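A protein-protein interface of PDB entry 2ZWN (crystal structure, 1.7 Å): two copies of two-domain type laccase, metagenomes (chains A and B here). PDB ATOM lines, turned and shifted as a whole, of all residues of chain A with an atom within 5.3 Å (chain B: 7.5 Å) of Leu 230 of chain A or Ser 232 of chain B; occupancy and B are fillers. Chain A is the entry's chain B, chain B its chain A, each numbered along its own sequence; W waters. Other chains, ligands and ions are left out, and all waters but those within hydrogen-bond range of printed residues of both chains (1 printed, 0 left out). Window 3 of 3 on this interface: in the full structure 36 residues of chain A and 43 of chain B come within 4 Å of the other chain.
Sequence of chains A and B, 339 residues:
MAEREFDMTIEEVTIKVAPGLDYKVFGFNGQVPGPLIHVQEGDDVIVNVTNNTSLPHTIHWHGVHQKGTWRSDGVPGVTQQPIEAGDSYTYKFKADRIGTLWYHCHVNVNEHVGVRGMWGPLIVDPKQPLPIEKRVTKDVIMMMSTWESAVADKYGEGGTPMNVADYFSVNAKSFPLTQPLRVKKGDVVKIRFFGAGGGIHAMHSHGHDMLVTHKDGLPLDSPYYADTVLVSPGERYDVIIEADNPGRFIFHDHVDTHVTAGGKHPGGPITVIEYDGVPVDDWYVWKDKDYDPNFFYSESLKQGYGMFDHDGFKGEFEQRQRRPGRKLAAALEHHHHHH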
ATOM      1  N   ILE A 200     -12.702  15.820 -19.816  1.00  0.00           N
ATOM      2  CA  ILE A 200     -12.412  17.125 -19.232  1.00  0.00           C
ATOM      3  C   ILE A 200     -13.718  17.765 -18.756  1.00  0.00           C
ATOM      4  O   ILE A 200     -14.732  17.706 -19.445  1.00  0.00           O
ATOM      5  CB  ILE A 200     -11.722  18.065 -20.240  1.00  0.00           C
ATOM      6  CG1 ILE A 200     -10.384  17.484 -20.699  1.00  0.00           C
ATOM      7  CG2 ILE A 200     -11.450  19.409 -19.608  1.00  0.00           C
ATOM      8  CD1 ILE A 200      -9.668  18.363 -21.721  1.00  0.00           C
ATOM      9  N   HIS A 201     -13.691  18.375 -17.580  1.00  0.00           N
ATOM     10  CA  HIS A 201     -14.900  18.895 -16.967  1.00  0.00           C
ATOM     11  C   HIS A 201     -14.651  20.326 -16.523  1.00  0.00           C
ATOM     12  O   HIS A 201     -13.640  20.599 -15.898  1.00  0.00           O
ATOM     13  CB  HIS A 201     -15.282  18.018 -15.782  1.00  0.00           C
ATOM     14  CG  HIS A 201     -15.457  16.577 -16.145  1.00  0.00           C
ATOM     15  ND1 HIS A 201     -16.661  16.055 -16.558  1.00  0.00           N
ATOM     16  CD2 HIS A 201     -14.567  15.558 -16.190  1.00  0.00           C
ATOM     17  CE1 HIS A 201     -16.510  14.770 -16.829  1.00  0.00           C
ATOM     18  NE2 HIS A 201     -15.248  14.444 -16.614  1.00  0.00           N
ATOM     19  N   ALA A 202     -15.573  21.223 -16.868  1.00  0.00           N
ATOM     20  CA  ALA A 202     -15.447  22.647 -16.560  1.00  0.00           C
ATOM     21  C   ALA A 202     -16.459  22.964 -15.477  1.00  0.00           C
ATOM     22  O   ALA A 202     -17.611  23.289 -15.757  1.00  0.00           O
ATOM     23  CB  ALA A 202     -15.708  23.492 -17.812  1.00  0.00           C
ATOM     24  N   MET A 203     -16.028  22.838 -14.228  1.00  0.00           N
ATOM     25  CA  MET A 203     -16.941  22.903 -13.089  1.00  0.00           C
ATOM     26  C   MET A 203     -17.259  24.343 -12.722  1.00  0.00           C
ATOM     27  O   MET A 203     -16.365  25.105 -12.356  1.00  0.00           O
ATOM     28  CB  MET A 203     -16.336  22.175 -11.886  1.00  0.00           C
ATOM     29  CG  MET A 203     -15.997  20.708 -12.165  1.00  0.00           C
ATOM     30  SD  MET A 203     -17.341  19.728 -12.863  1.00  0.00           S
ATOM     31  CE  MET A 203     -18.511  19.707 -11.495  1.00  0.00           C
ATOM     32  N   THR A 228     -15.291  29.093 -12.884  1.00  0.00           N
ATOM     33  CA  THR A 228     -15.254  27.858 -13.669  1.00  0.00           C
ATOM     34  C   THR A 228     -13.855  27.251 -13.562  1.00  0.00           C
ATOM     35  O   THR A 228     -12.870  27.925 -13.857  1.00  0.00           O
ATOM     36  CB  THR A 228     -15.616  28.145 -15.144  1.00  0.00           C
ATOM     37  OG1 THR A 228     -16.904  28.774 -15.206  1.00  0.00           O
ATOM     38  CG2 THR A 228     -15.638  26.860 -15.981  1.00  0.00           C
ATOM     39  N   VAL A 229     -13.770  25.999 -13.111  1.00  0.00           N
ATOM     40  CA  VAL A 229     -12.488  25.310 -12.917  1.00  0.00           C
ATOM     41  C   VAL A 229     -12.392  24.118 -13.867  1.00  0.00           C
ATOM     42  O   VAL A 229     -13.195  23.195 -13.778  1.00  0.00           O
ATOM     43  CB  VAL A 229     -12.337  24.811 -11.461  1.00  0.00           C
ATOM     44  CG1 VAL A 229     -11.009  24.055 -11.271  1.00  0.00           C
ATOM     45  CG2 VAL A 229     -12.421  25.976 -10.505  1.00  0.00           C
ATOM     46  N   LEU A 230     -11.417  24.139 -14.769  1.00  0.00           N
ATOM     47  CA  LEU A 230     -11.223  23.040 -15.720  1.00  0.00           C
ATOM     48  C   LEU A 230     -10.453  21.896 -15.041  1.00  0.00           C
ATOM     49  O   LEU A 230      -9.339  22.095 -14.534  1.00  0.00           O
ATOM     50  CB  LEU A 230     -10.486  23.511 -16.980  1.00  0.00           C
ATOM     51  CG  LEU A 230     -10.430  22.506 -18.138  1.00  0.00           C
ATOM     52  CD1 LEU A 230     -11.840  22.238 -18.665  1.00  0.00           C
ATOM     53  CD2 LEU A 230      -9.505  22.998 -19.252  1.00  0.00           C
ATOM     54  N   VAL A 231     -11.058  20.711 -15.040  1.00  0.00           N
ATOM     55  CA  VAL A 231     -10.471  19.518 -14.424  1.00  0.00           C
ATOM     56  C   VAL A 231     -10.274  18.459 -15.501  1.00  0.00           C
ATOM     57  O   VAL A 231     -11.237  18.071 -16.165  1.00  0.00           O
ATOM     58  CB  VAL A 231     -11.391  18.957 -13.321  1.00  0.00           C
ATOM     59  CG1 VAL A 231     -10.704  17.816 -12.582  1.00  0.00           C
ATOM     60  CG2 VAL A 231     -11.783  20.061 -12.337  1.00  0.00           C
ATOM     61  N   SER A 232      -9.035  18.012 -15.688  1.00  0.00           N
ATOM     62  CA  SER A 232      -8.714  17.036 -16.724  1.00  0.00           C
ATOM     63  C   SER A 232      -8.204  15.738 -16.089  1.00  0.00           C
ATOM     64  O   SER A 232      -7.938  15.705 -14.886  1.00  0.00           O
ATOM     65  CB  SER A 232      -7.709  17.626 -17.722  1.00  0.00           C
ATOM     66  OG  SER A 232      -6.376  17.553 -17.260  1.00  0.00           O
ATOM     67  N   GLU A 235      -5.946  15.040 -12.727  1.00  0.00           N
ATOM     68  CA  GLU A 235      -5.780  16.252 -11.919  1.00  0.00           C
ATOM     69  C   GLU A 235      -6.710  16.288 -10.721  1.00  0.00           C
ATOM     70  O   GLU A 235      -7.791  15.696 -10.736  1.00  0.00           O
ATOM     71  CB  GLU A 235      -6.070  17.498 -12.753  1.00  0.00           C
ATOM     72  CG  GLU A 235      -5.176  17.725 -13.936  1.00  0.00           C
ATOM     73  CD  GLU A 235      -5.416  19.100 -14.510  1.00  0.00           C
ATOM     74  OE1 GLU A 235      -6.471  19.281 -15.153  1.00  0.00           O
ATOM     75  OE2 GLU A 235      -4.586  20.002 -14.265  1.00  0.00           O
ATOM     76  N   TYR A 237      -8.158  19.583  -8.066  1.00  0.00           N
ATOM     77  CA  TYR A 237      -8.176  20.968  -7.619  1.00  0.00           C
ATOM     78  C   TYR A 237      -8.998  21.050  -6.344  1.00  0.00           C
ATOM     79  O   TYR A 237     -10.085  20.477  -6.275  1.00  0.00           O
ATOM     80  CB  TYR A 237      -8.780  21.880  -8.694  1.00  0.00           C
ATOM     81  CG  TYR A 237      -7.870  22.066  -9.883  1.00  0.00           C
ATOM     82  CD1 TYR A 237      -6.948  23.108  -9.920  1.00  0.00           C
ATOM     83  CD2 TYR A 237      -7.905  21.181 -10.953  1.00  0.00           C
ATOM     84  CE1 TYR A 237      -6.098  23.273 -11.014  1.00  0.00           C
ATOM     85  CE2 TYR A 237      -7.059  21.335 -12.043  1.00  0.00           C
ATOM     86  CZ  TYR A 237      -6.158  22.378 -12.070  1.00  0.00           C
ATOM     87  OH  TYR A 237      -5.315  22.524 -13.158  1.00  0.00           O
ATOM     88  N   TRP B 102     -20.599  37.081 -18.666  1.00  0.00           N
ATOM     89  CA  TRP B 102     -21.402  36.856 -19.858  1.00  0.00           C
ATOM     90  C   TRP B 102     -22.788  36.362 -19.495  1.00  0.00           C
ATOM     91  O   TRP B 102     -23.090  36.126 -18.326  1.00  0.00           O
ATOM     92  CB  TRP B 102     -20.678  35.931 -20.846  1.00  0.00           C
ATOM     93  CG  TRP B 102     -20.431  34.513 -20.416  1.00  0.00           C
ATOM     94  CD1 TRP B 102     -19.792  34.084 -19.290  1.00  0.00           C
ATOM     95  CD2 TRP B 102     -20.768  33.338 -21.159  1.00  0.00           C
ATOM     96  NE1 TRP B 102     -19.739  32.706 -19.274  1.00  0.00           N
ATOM     97  CE2 TRP B 102     -20.330  32.226 -20.411  1.00  0.00           C
ATOM     98  CE3 TRP B 102     -21.418  33.117 -22.380  1.00  0.00           C
ATOM     99  CZ2 TRP B 102     -20.523  30.913 -20.844  1.00  0.00           C
ATOM    100  CZ3 TRP B 102     -21.608  31.821 -22.807  1.00  0.00           C
ATOM    101  CH2 TRP B 102     -21.154  30.731 -22.043  1.00  0.00           C
ATOM    102  N   PHE B 193     -11.184  36.784 -23.762  1.00  0.00           N
ATOM    103  CA  PHE B 193     -11.545  35.507 -24.380  1.00  0.00           C
ATOM    104  C   PHE B 193     -12.689  34.862 -23.606  1.00  0.00           C
ATOM    105  O   PHE B 193     -12.651  34.818 -22.374  1.00  0.00           O
ATOM    106  CB  PHE B 193     -10.377  34.526 -24.313  1.00  0.00           C
ATOM    107  CG  PHE B 193      -9.139  34.953 -25.054  1.00  0.00           C
ATOM    108  CD1 PHE B 193      -9.152  35.137 -26.437  1.00  0.00           C
ATOM    109  CD2 PHE B 193      -7.932  35.078 -24.380  1.00  0.00           C
ATOM    110  CE1 PHE B 193      -7.987  35.494 -27.117  1.00  0.00           C
ATOM    111  CE2 PHE B 193      -6.768  35.437 -25.051  1.00  0.00           C
ATOM    112  CZ  PHE B 193      -6.795  35.639 -26.419  1.00  0.00           C
ATOM    113  N   PHE B 194     -13.673  34.323 -24.325  1.00  0.00           N
ATOM    114  CA  PHE B 194     -14.804  33.616 -23.715  1.00  0.00           C
ATOM    115  C   PHE B 194     -14.935  32.218 -24.318  1.00  0.00           C
ATOM    116  O   PHE B 194     -14.950  32.070 -25.541  1.00  0.00           O
ATOM    117  CB  PHE B 194     -16.137  34.312 -24.003  1.00  0.00           C
ATOM    118  CG  PHE B 194     -16.225  35.753 -23.554  1.00  0.00           C
ATOM    119  CD1 PHE B 194     -17.160  36.127 -22.599  1.00  0.00           C
ATOM    120  CD2 PHE B 194     -15.453  36.742 -24.155  1.00  0.00           C
ATOM    121  CE1 PHE B 194     -17.281  37.456 -22.201  1.00  0.00           C
ATOM    122  CE2 PHE B 194     -15.570  38.074 -23.764  1.00  0.00           C
ATOM    123  CZ  PHE B 194     -16.495  38.430 -22.795  1.00  0.00           C
ATOM    124  N   GLY B 195     -15.068  31.206 -23.465  1.00  0.00           N
ATOM    125  CA  GLY B 195     -15.471  29.870 -23.905  1.00  0.00           C
ATOM    126  C   GLY B 195     -16.991  29.803 -23.975  1.00  0.00           C
ATOM    127  O   GLY B 195     -17.645  29.264 -23.082  1.00  0.00           O
ATOM    128  N   ALA B 196     -17.551  30.353 -25.048  1.00  0.00           N
ATOM    129  CA  ALA B 196     -19.004  30.504 -25.157  1.00  0.00           C
ATOM    130  C   ALA B 196     -19.702  29.187 -25.494  1.00  0.00           C
ATOM    131  O   ALA B 196     -20.744  28.877 -24.907  1.00  0.00           O
ATOM    132  CB  ALA B 196     -19.351  31.587 -26.175  1.00  0.00           C
ATOM    133  N   GLY B 197     -19.136  28.421 -26.429  1.00  0.00           N
ATOM    134  CA  GLY B 197     -19.676  27.117 -26.815  1.00  0.00           C
ATOM    135  C   GLY B 197     -19.095  25.937 -26.046  1.00  0.00           C
ATOM    136  O   GLY B 197     -18.552  26.090 -24.946  1.00  0.00           O
ATOM    137  N   GLY B 198     -19.187  24.754 -26.645  1.00  0.00           N
ATOM    138  CA  GLY B 198     -18.820  23.507 -25.972  1.00  0.00           C
ATOM    139  C   GLY B 198     -17.404  23.013 -26.226  1.00  0.00           C
ATOM    140  O   GLY B 198     -17.042  21.921 -25.777  1.00  0.00           O
ATOM    141  N   GLY B 199     -16.601  23.808 -26.932  1.00  0.00           N
ATOM    142  CA  GLY B 199     -15.247  23.404 -27.329  1.00  0.00           C
ATOM    143  C   GLY B 199     -14.145  23.976 -26.453  1.00  0.00           C
ATOM    144  O   GLY B 199     -14.389  24.844 -25.616  1.00  0.00           O
ATOM    145  N   ILE B 200     -12.929  23.473 -26.652  1.00  0.00           N
ATOM    146  CA  ILE B 200     -11.733  24.025 -26.027  1.00  0.00           C
ATOM    147  C   ILE B 200     -10.919  24.674 -27.138  1.00  0.00           C
ATOM    148  O   ILE B 200     -10.800  24.117 -28.227  1.00  0.00           O
ATOM    149  CB  ILE B 200     -10.903  22.932 -25.321  1.00  0.00           C
ATOM    150  CG1 ILE B 200     -11.679  22.370 -24.133  1.00  0.00           C
ATOM    151  CG2 ILE B 200      -9.568  23.480 -24.860  1.00  0.00           C
ATOM    152  CD1 ILE B 200     -11.056  21.136 -23.536  1.00  0.00           C
ATOM    153  N   HIS B 201     -10.374  25.856 -26.865  1.00  0.00           N
ATOM    154  CA  HIS B 201      -9.723  26.664 -27.885  1.00  0.00           C
ATOM    155  C   HIS B 201      -8.384  27.141 -27.350  1.00  0.00           C
ATOM    156  O   HIS B 201      -8.326  27.702 -26.257  1.00  0.00           O
ATOM    157  CB  HIS B 201     -10.608  27.859 -28.235  1.00  0.00           C
ATOM    158  CG  HIS B 201     -11.977  27.473 -28.698  1.00  0.00           C
ATOM    159  ND1 HIS B 201     -12.280  27.246 -30.024  1.00  0.00           N
ATOM    160  CD2 HIS B 201     -13.116  27.241 -28.005  1.00  0.00           C
ATOM    161  CE1 HIS B 201     -13.553  26.901 -30.127  1.00  0.00           C
ATOM    162  NE2 HIS B 201     -14.082  26.892 -28.916  1.00  0.00           N
ATOM    163  N   ALA B 202      -7.318  26.909 -28.109  1.00  0.00           N
ATOM    164  CA  ALA B 202      -5.970  27.280 -27.684  1.00  0.00           C
ATOM    165  C   ALA B 202      -5.546  28.517 -28.469  1.00  0.00           C
ATOM    166  O   ALA B 202      -5.050  28.420 -29.588  1.00  0.00           O
ATOM    167  CB  ALA B 202      -5.001  26.118 -27.911  1.00  0.00           C
ATOM    168  N   LYS B 215      -8.679  36.000 -14.604  1.00  0.00           N
ATOM    169  CA  LYS B 215      -9.348  34.727 -14.826  1.00  0.00           C
ATOM    170  C   LYS B 215     -10.802  34.895 -14.380  1.00  0.00           C
ATOM    171  O   LYS B 215     -11.064  35.332 -13.251  1.00  0.00           O
ATOM    172  CB  LYS B 215      -8.615  33.625 -14.052  1.00  0.00           C
ATOM    173  CG  LYS B 215      -9.408  32.405 -13.678  1.00  0.00           C
ATOM    174  CD  LYS B 215      -9.899  31.612 -14.861  1.00  0.00           C
ATOM    175  CE  LYS B 215     -10.553  30.320 -14.366  1.00  0.00           C
ATOM    176  NZ  LYS B 215     -11.480  29.727 -15.355  1.00  0.00           N
ATOM    177  N   ASP B 216     -11.730  34.569 -15.279  1.00  0.00           N
ATOM    178  CA  ASP B 216     -13.167  34.723 -15.049  1.00  0.00           C
ATOM    179  C   ASP B 216     -13.527  36.127 -14.548  1.00  0.00           C
ATOM    180  O   ASP B 216     -14.413  36.293 -13.716  1.00  0.00           O
ATOM    181  CB  ASP B 216     -13.666  33.646 -14.080  1.00  0.00           C
ATOM    182  CG  ASP B 216     -13.451  32.229 -14.615  1.00  0.00           C
ATOM    183  OD1 ASP B 216     -13.232  32.069 -15.840  1.00  0.00           O
ATOM    184  OD2 ASP B 216     -13.512  31.283 -13.803  1.00  0.00           O
ATOM    185  N   VAL B 229      -3.166  30.623 -24.959  1.00  0.00           N
ATOM    186  CA  VAL B 229      -4.066  30.581 -23.807  1.00  0.00           C
ATOM    187  C   VAL B 229      -5.210  29.615 -24.086  1.00  0.00           C
ATOM    188  O   VAL B 229      -5.969  29.806 -25.035  1.00  0.00           O
ATOM    189  CB  VAL B 229      -4.636  31.976 -23.493  1.00  0.00           C
ATOM    190  CG1 VAL B 229      -5.661  31.900 -22.359  1.00  0.00           C
ATOM    191  CG2 VAL B 229      -3.498  32.939 -23.143  1.00  0.00           C
ATOM    192  N   LEU B 230      -5.301  28.568 -23.268  1.00  0.00           N
ATOM    193  CA  LEU B 230      -6.352  27.563 -23.394  1.00  0.00           C
ATOM    194  C   LEU B 230      -7.637  28.072 -22.758  1.00  0.00           C
ATOM    195  O   LEU B 230      -7.664  28.377 -21.559  1.00  0.00           O
ATOM    196  CB  LEU B 230      -5.930  26.263 -22.720  1.00  0.00           C
ATOM    197  CG  LEU B 230      -6.856  25.066 -22.923  1.00  0.00           C
ATOM    198  CD1 LEU B 230      -6.820  24.637 -24.391  1.00  0.00           C
ATOM    199  CD2 LEU B 230      -6.469  23.913 -21.992  1.00  0.00           C
ATOM    200  N   VAL B 231      -8.694  28.139 -23.563  1.00  0.00           N
ATOM    201  CA  VAL B 231      -9.992  28.648 -23.124  1.00  0.00           C
ATOM    202  C   VAL B 231     -11.014  27.524 -23.262  1.00  0.00           C
ATOM    203  O   VAL B 231     -11.209  27.002 -24.362  1.00  0.00           O
ATOM    204  CB  VAL B 231     -10.421  29.864 -23.961  1.00  0.00           C
ATOM    205  CG1 VAL B 231     -11.692  30.485 -23.397  1.00  0.00           C
ATOM    206  CG2 VAL B 231      -9.299  30.920 -23.999  1.00  0.00           C
ATOM    207  N   SER B 232     -11.646  27.153 -22.148  1.00  0.00           N
ATOM    208  CA  SER B 232     -12.607  26.042 -22.122  1.00  0.00           C
ATOM    209  C   SER B 232     -14.009  26.567 -21.787  1.00  0.00           C
ATOM    210  O   SER B 232     -14.147  27.726 -21.377  1.00  0.00           O
ATOM    211  CB  SER B 232     -12.153  24.956 -21.139  1.00  0.00           C
ATOM    212  OG  SER B 232     -12.563  25.228 -19.812  1.00  0.00           O
ATOM    213  N   PRO B 233     -15.049  25.732 -21.983  1.00  0.00           N
ATOM    214  CA  PRO B 233     -16.426  26.202 -21.807  1.00  0.00           C
ATOM    215  C   PRO B 233     -16.695  26.875 -20.458  1.00  0.00           C
ATOM    216  O   PRO B 233     -16.402  26.303 -19.406  1.00  0.00           O
ATOM    217  CB  PRO B 233     -17.254  24.922 -21.961  1.00  0.00           C
ATOM    218  CG  PRO B 233     -16.434  24.085 -22.883  1.00  0.00           C
ATOM    219  CD  PRO B 233     -15.021  24.322 -22.412  1.00  0.00           C
ATOM    220  N   GLY B 234     -17.253  28.080 -20.515  1.00  0.00           N
ATOM    221  CA  GLY B 234     -17.616  28.840 -19.323  1.00  0.00           C
ATOM    222  C   GLY B 234     -16.559  29.825 -18.884  1.00  0.00           C
ATOM    223  O   GLY B 234     -16.883  30.822 -18.239  1.00  0.00           O
ATOM    224  N   GLU B 235     -15.299  29.562 -19.226  1.00  0.00           N
ATOM    225  CA  GLU B 235     -14.193  30.386 -18.745  1.00  0.00           C
ATOM    226  C   GLU B 235     -14.062  31.708 -19.480  1.00  0.00           C
ATOM    227  O   GLU B 235     -14.459  31.830 -20.638  1.00  0.00           O
ATOM    228  CB  GLU B 235     -12.866  29.663 -18.932  1.00  0.00           C
ATOM    229  CG  GLU B 235     -12.696  28.368 -18.187  1.00  0.00           C
ATOM    230  CD  GLU B 235     -11.250  27.924 -18.241  1.00  0.00           C
ATOM    231  OE1 GLU B 235     -10.823  27.449 -19.312  1.00  0.00           O
ATOM    232  OE2 GLU B 235     -10.529  28.087 -17.238  1.00  0.00           O
ATOM    233  N   ARG B 236     -13.482  32.691 -18.796  1.00  0.00           N
ATOM    234  CA  ARG B 236     -12.965  33.887 -19.462  1.00  0.00           C
ATOM    235  C   ARG B 236     -11.538  34.152 -19.005  1.00  0.00           C
ATOM    236  O   ARG B 236     -11.175  33.883 -17.850  1.00  0.00           O
ATOM    237  CB  ARG B 236     -13.834  35.119 -19.200  1.00  0.00           C
ATOM    238  CG  ARG B 236     -15.194  35.108 -19.891  1.00  0.00           C
ATOM    239  CD  ARG B 236     -16.232  34.374 -19.072  1.00  0.00           C
ATOM    240  NE  ARG B 236     -16.479  35.059 -17.803  1.00  0.00           N
ATOM    241  CZ  ARG B 236     -16.677  34.464 -16.630  1.00  0.00           C
ATOM    242  NH1 ARG B 236     -16.685  33.146 -16.517  1.00  0.00           N
ATOM    243  NH2 ARG B 236     -16.858  35.209 -15.550  1.00  0.00           N
ATOM    244  N   TYR B 237     -10.725  34.637 -19.934  1.00  0.00           N
ATOM    245  CA  TYR B 237      -9.393  35.149 -19.630  1.00  0.00           C
ATOM    246  C   TYR B 237      -9.274  36.532 -20.230  1.00  0.00           C
ATOM    247  O   TYR B 237      -9.700  36.746 -21.364  1.00  0.00           O
ATOM    248  CB  TYR B 237      -8.313  34.239 -20.211  1.00  0.00           C
ATOM    249  CG  TYR B 237      -8.221  32.919 -19.493  1.00  0.00           C
ATOM    250  CD1 TYR B 237      -7.361  32.753 -18.421  1.00  0.00           C
ATOM    251  CD2 TYR B 237      -9.017  31.847 -19.873  1.00  0.00           C
ATOM    252  CE1 TYR B 237      -7.281  31.549 -17.748  1.00  0.00           C
ATOM    253  CE2 TYR B 237      -8.946  30.633 -19.208  1.00  0.00           C
ATOM    254  CZ  TYR B 237      -8.080  30.492 -18.147  1.00  0.00           C
ATOM    255  OH  TYR B 237      -8.007  29.289 -17.475  1.00  0.00           O
HETATM  256  O   HOH W   1      -9.615  26.487 -15.227  1.00  0.00           O
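O of Gly 195 of chain B lies within hydrogen-bond range of N of Gly 234 of chain B, 2.9 Å away.
The backbone carbonyl oxygen (O) of Glu 235 of chain B lies within hydrogen-bond range of the backbone NH (N) of Gly 195 of chain B (3.0 Å).
The side-chain amino group of Lys 215 of chain B lies within salt-bridge range of the side-chain carboxylate of Asp 216 of chain B (3.0 Å).
The side-chain carboxylate (OD1) of Asp 216 of chain B lies within salt-bridge range of the guanidinium group (NH1) of Arg 236 of chain B (3.7 Å).
The guanidinium group (NH1) of Arg 236 of chain B is in hydrogen-bond range of the backbone carbonyl oxygen (O) of Gly 234 of chain B (2.9 Å).
The side-chain hydroxyl (OH) of Tyr 237 of chain B lies within hydrogen-bond range of the side-chain carboxylate (OE2) of Glu 235 of chain B (2.8 Å).
Leu 230 of chain A touches one residue of chain B.
Ser 232 of chain B touches one residue of chain A.
Of the printed residues of chain A, Ile 200 of chain B touches Ile 200.
Printed residues of chain A within 4 Å of Asp 216 of chain B: Thr 228.
Of the printed residues of chain A, Gly 234 of chain B touches Thr 228 (3.7 Å).
Printed residues of chain A within 4 Å of Lys 215 of chain B: Thr 228 (2.7 Å).
Printed residues of chain A within 4 Å of Pro 233 of chain B: Ala 202 and Thr 228.
Phe 193 of chain B touches none of the printed residues of chain A.
Arg 236 of chain B touches none of the printed residues of chain A.
The nearest residue of chain B that does not touch Leu 230 of chain A is Leu 230 of chain B (4.2 Å).
The nearest residue of chain A that does not touch Ser 232 of chain B is Ala 202 of chain A (4.1 Å).
Ile 200 of chain B touches Ile 200 of chain A.
Pro 233 of chain B touches Ala 202 of chain A.
Thr 228 of chain A touches Pro 233 of chain B.
Thr 228 of chain A touches Gly 234 of chain B (OG1 to O, 3.7 Å).
Glu 235 of chain B touches Thr 228 of chain A (CG to CG2, 3.97 Å).
Ser 232 of chain B touches Leu 230 of chain A.
Water W1 lies within hydrogen-bond range of the side-chain carboxylate (OE2) of Glu 235 of chain B (2.7 Å) and the backbone NH (N) of Leu 230 of chain A (3.0 Å).
Ile 200 of chain A touches its own counterpart, Ile 200 of chain B.
Leu 230 of chain A touches Ser 232 of chain B, but with the chains exchanged Ser 232 of chain A does not touch Leu 230 of chain B (7.7 Å).
9 positions are printed for both chains.
Printed residues of chain A that touch a printed residue of chain B: Ile 200, Ala 202, Thr 228 and Leu 230.
Hydrophobic or aromatic side chains of chain A within 4 Å of the printed part of chain B: Ile 200, Ala 202 and Leu 230.
Among the printed residues, 8 pairs touch across the chains.
Among the printed residues, no Asp or Glu carboxylate lies within 4 Å of a Lys or Arg side-chain nitrogen of the other chain.
The backbone carbonyl oxygen (O) of Thr 228 of chain A sits at hydrogen-bond distance from the side-chain amino group (NZ) of Lys 215 of chain B, at 2.7 Å.
N of Thr 228 of chain A lies within hydrogen-bond range of OD2 of Asp 216 of chain B, 3.0 Å away.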
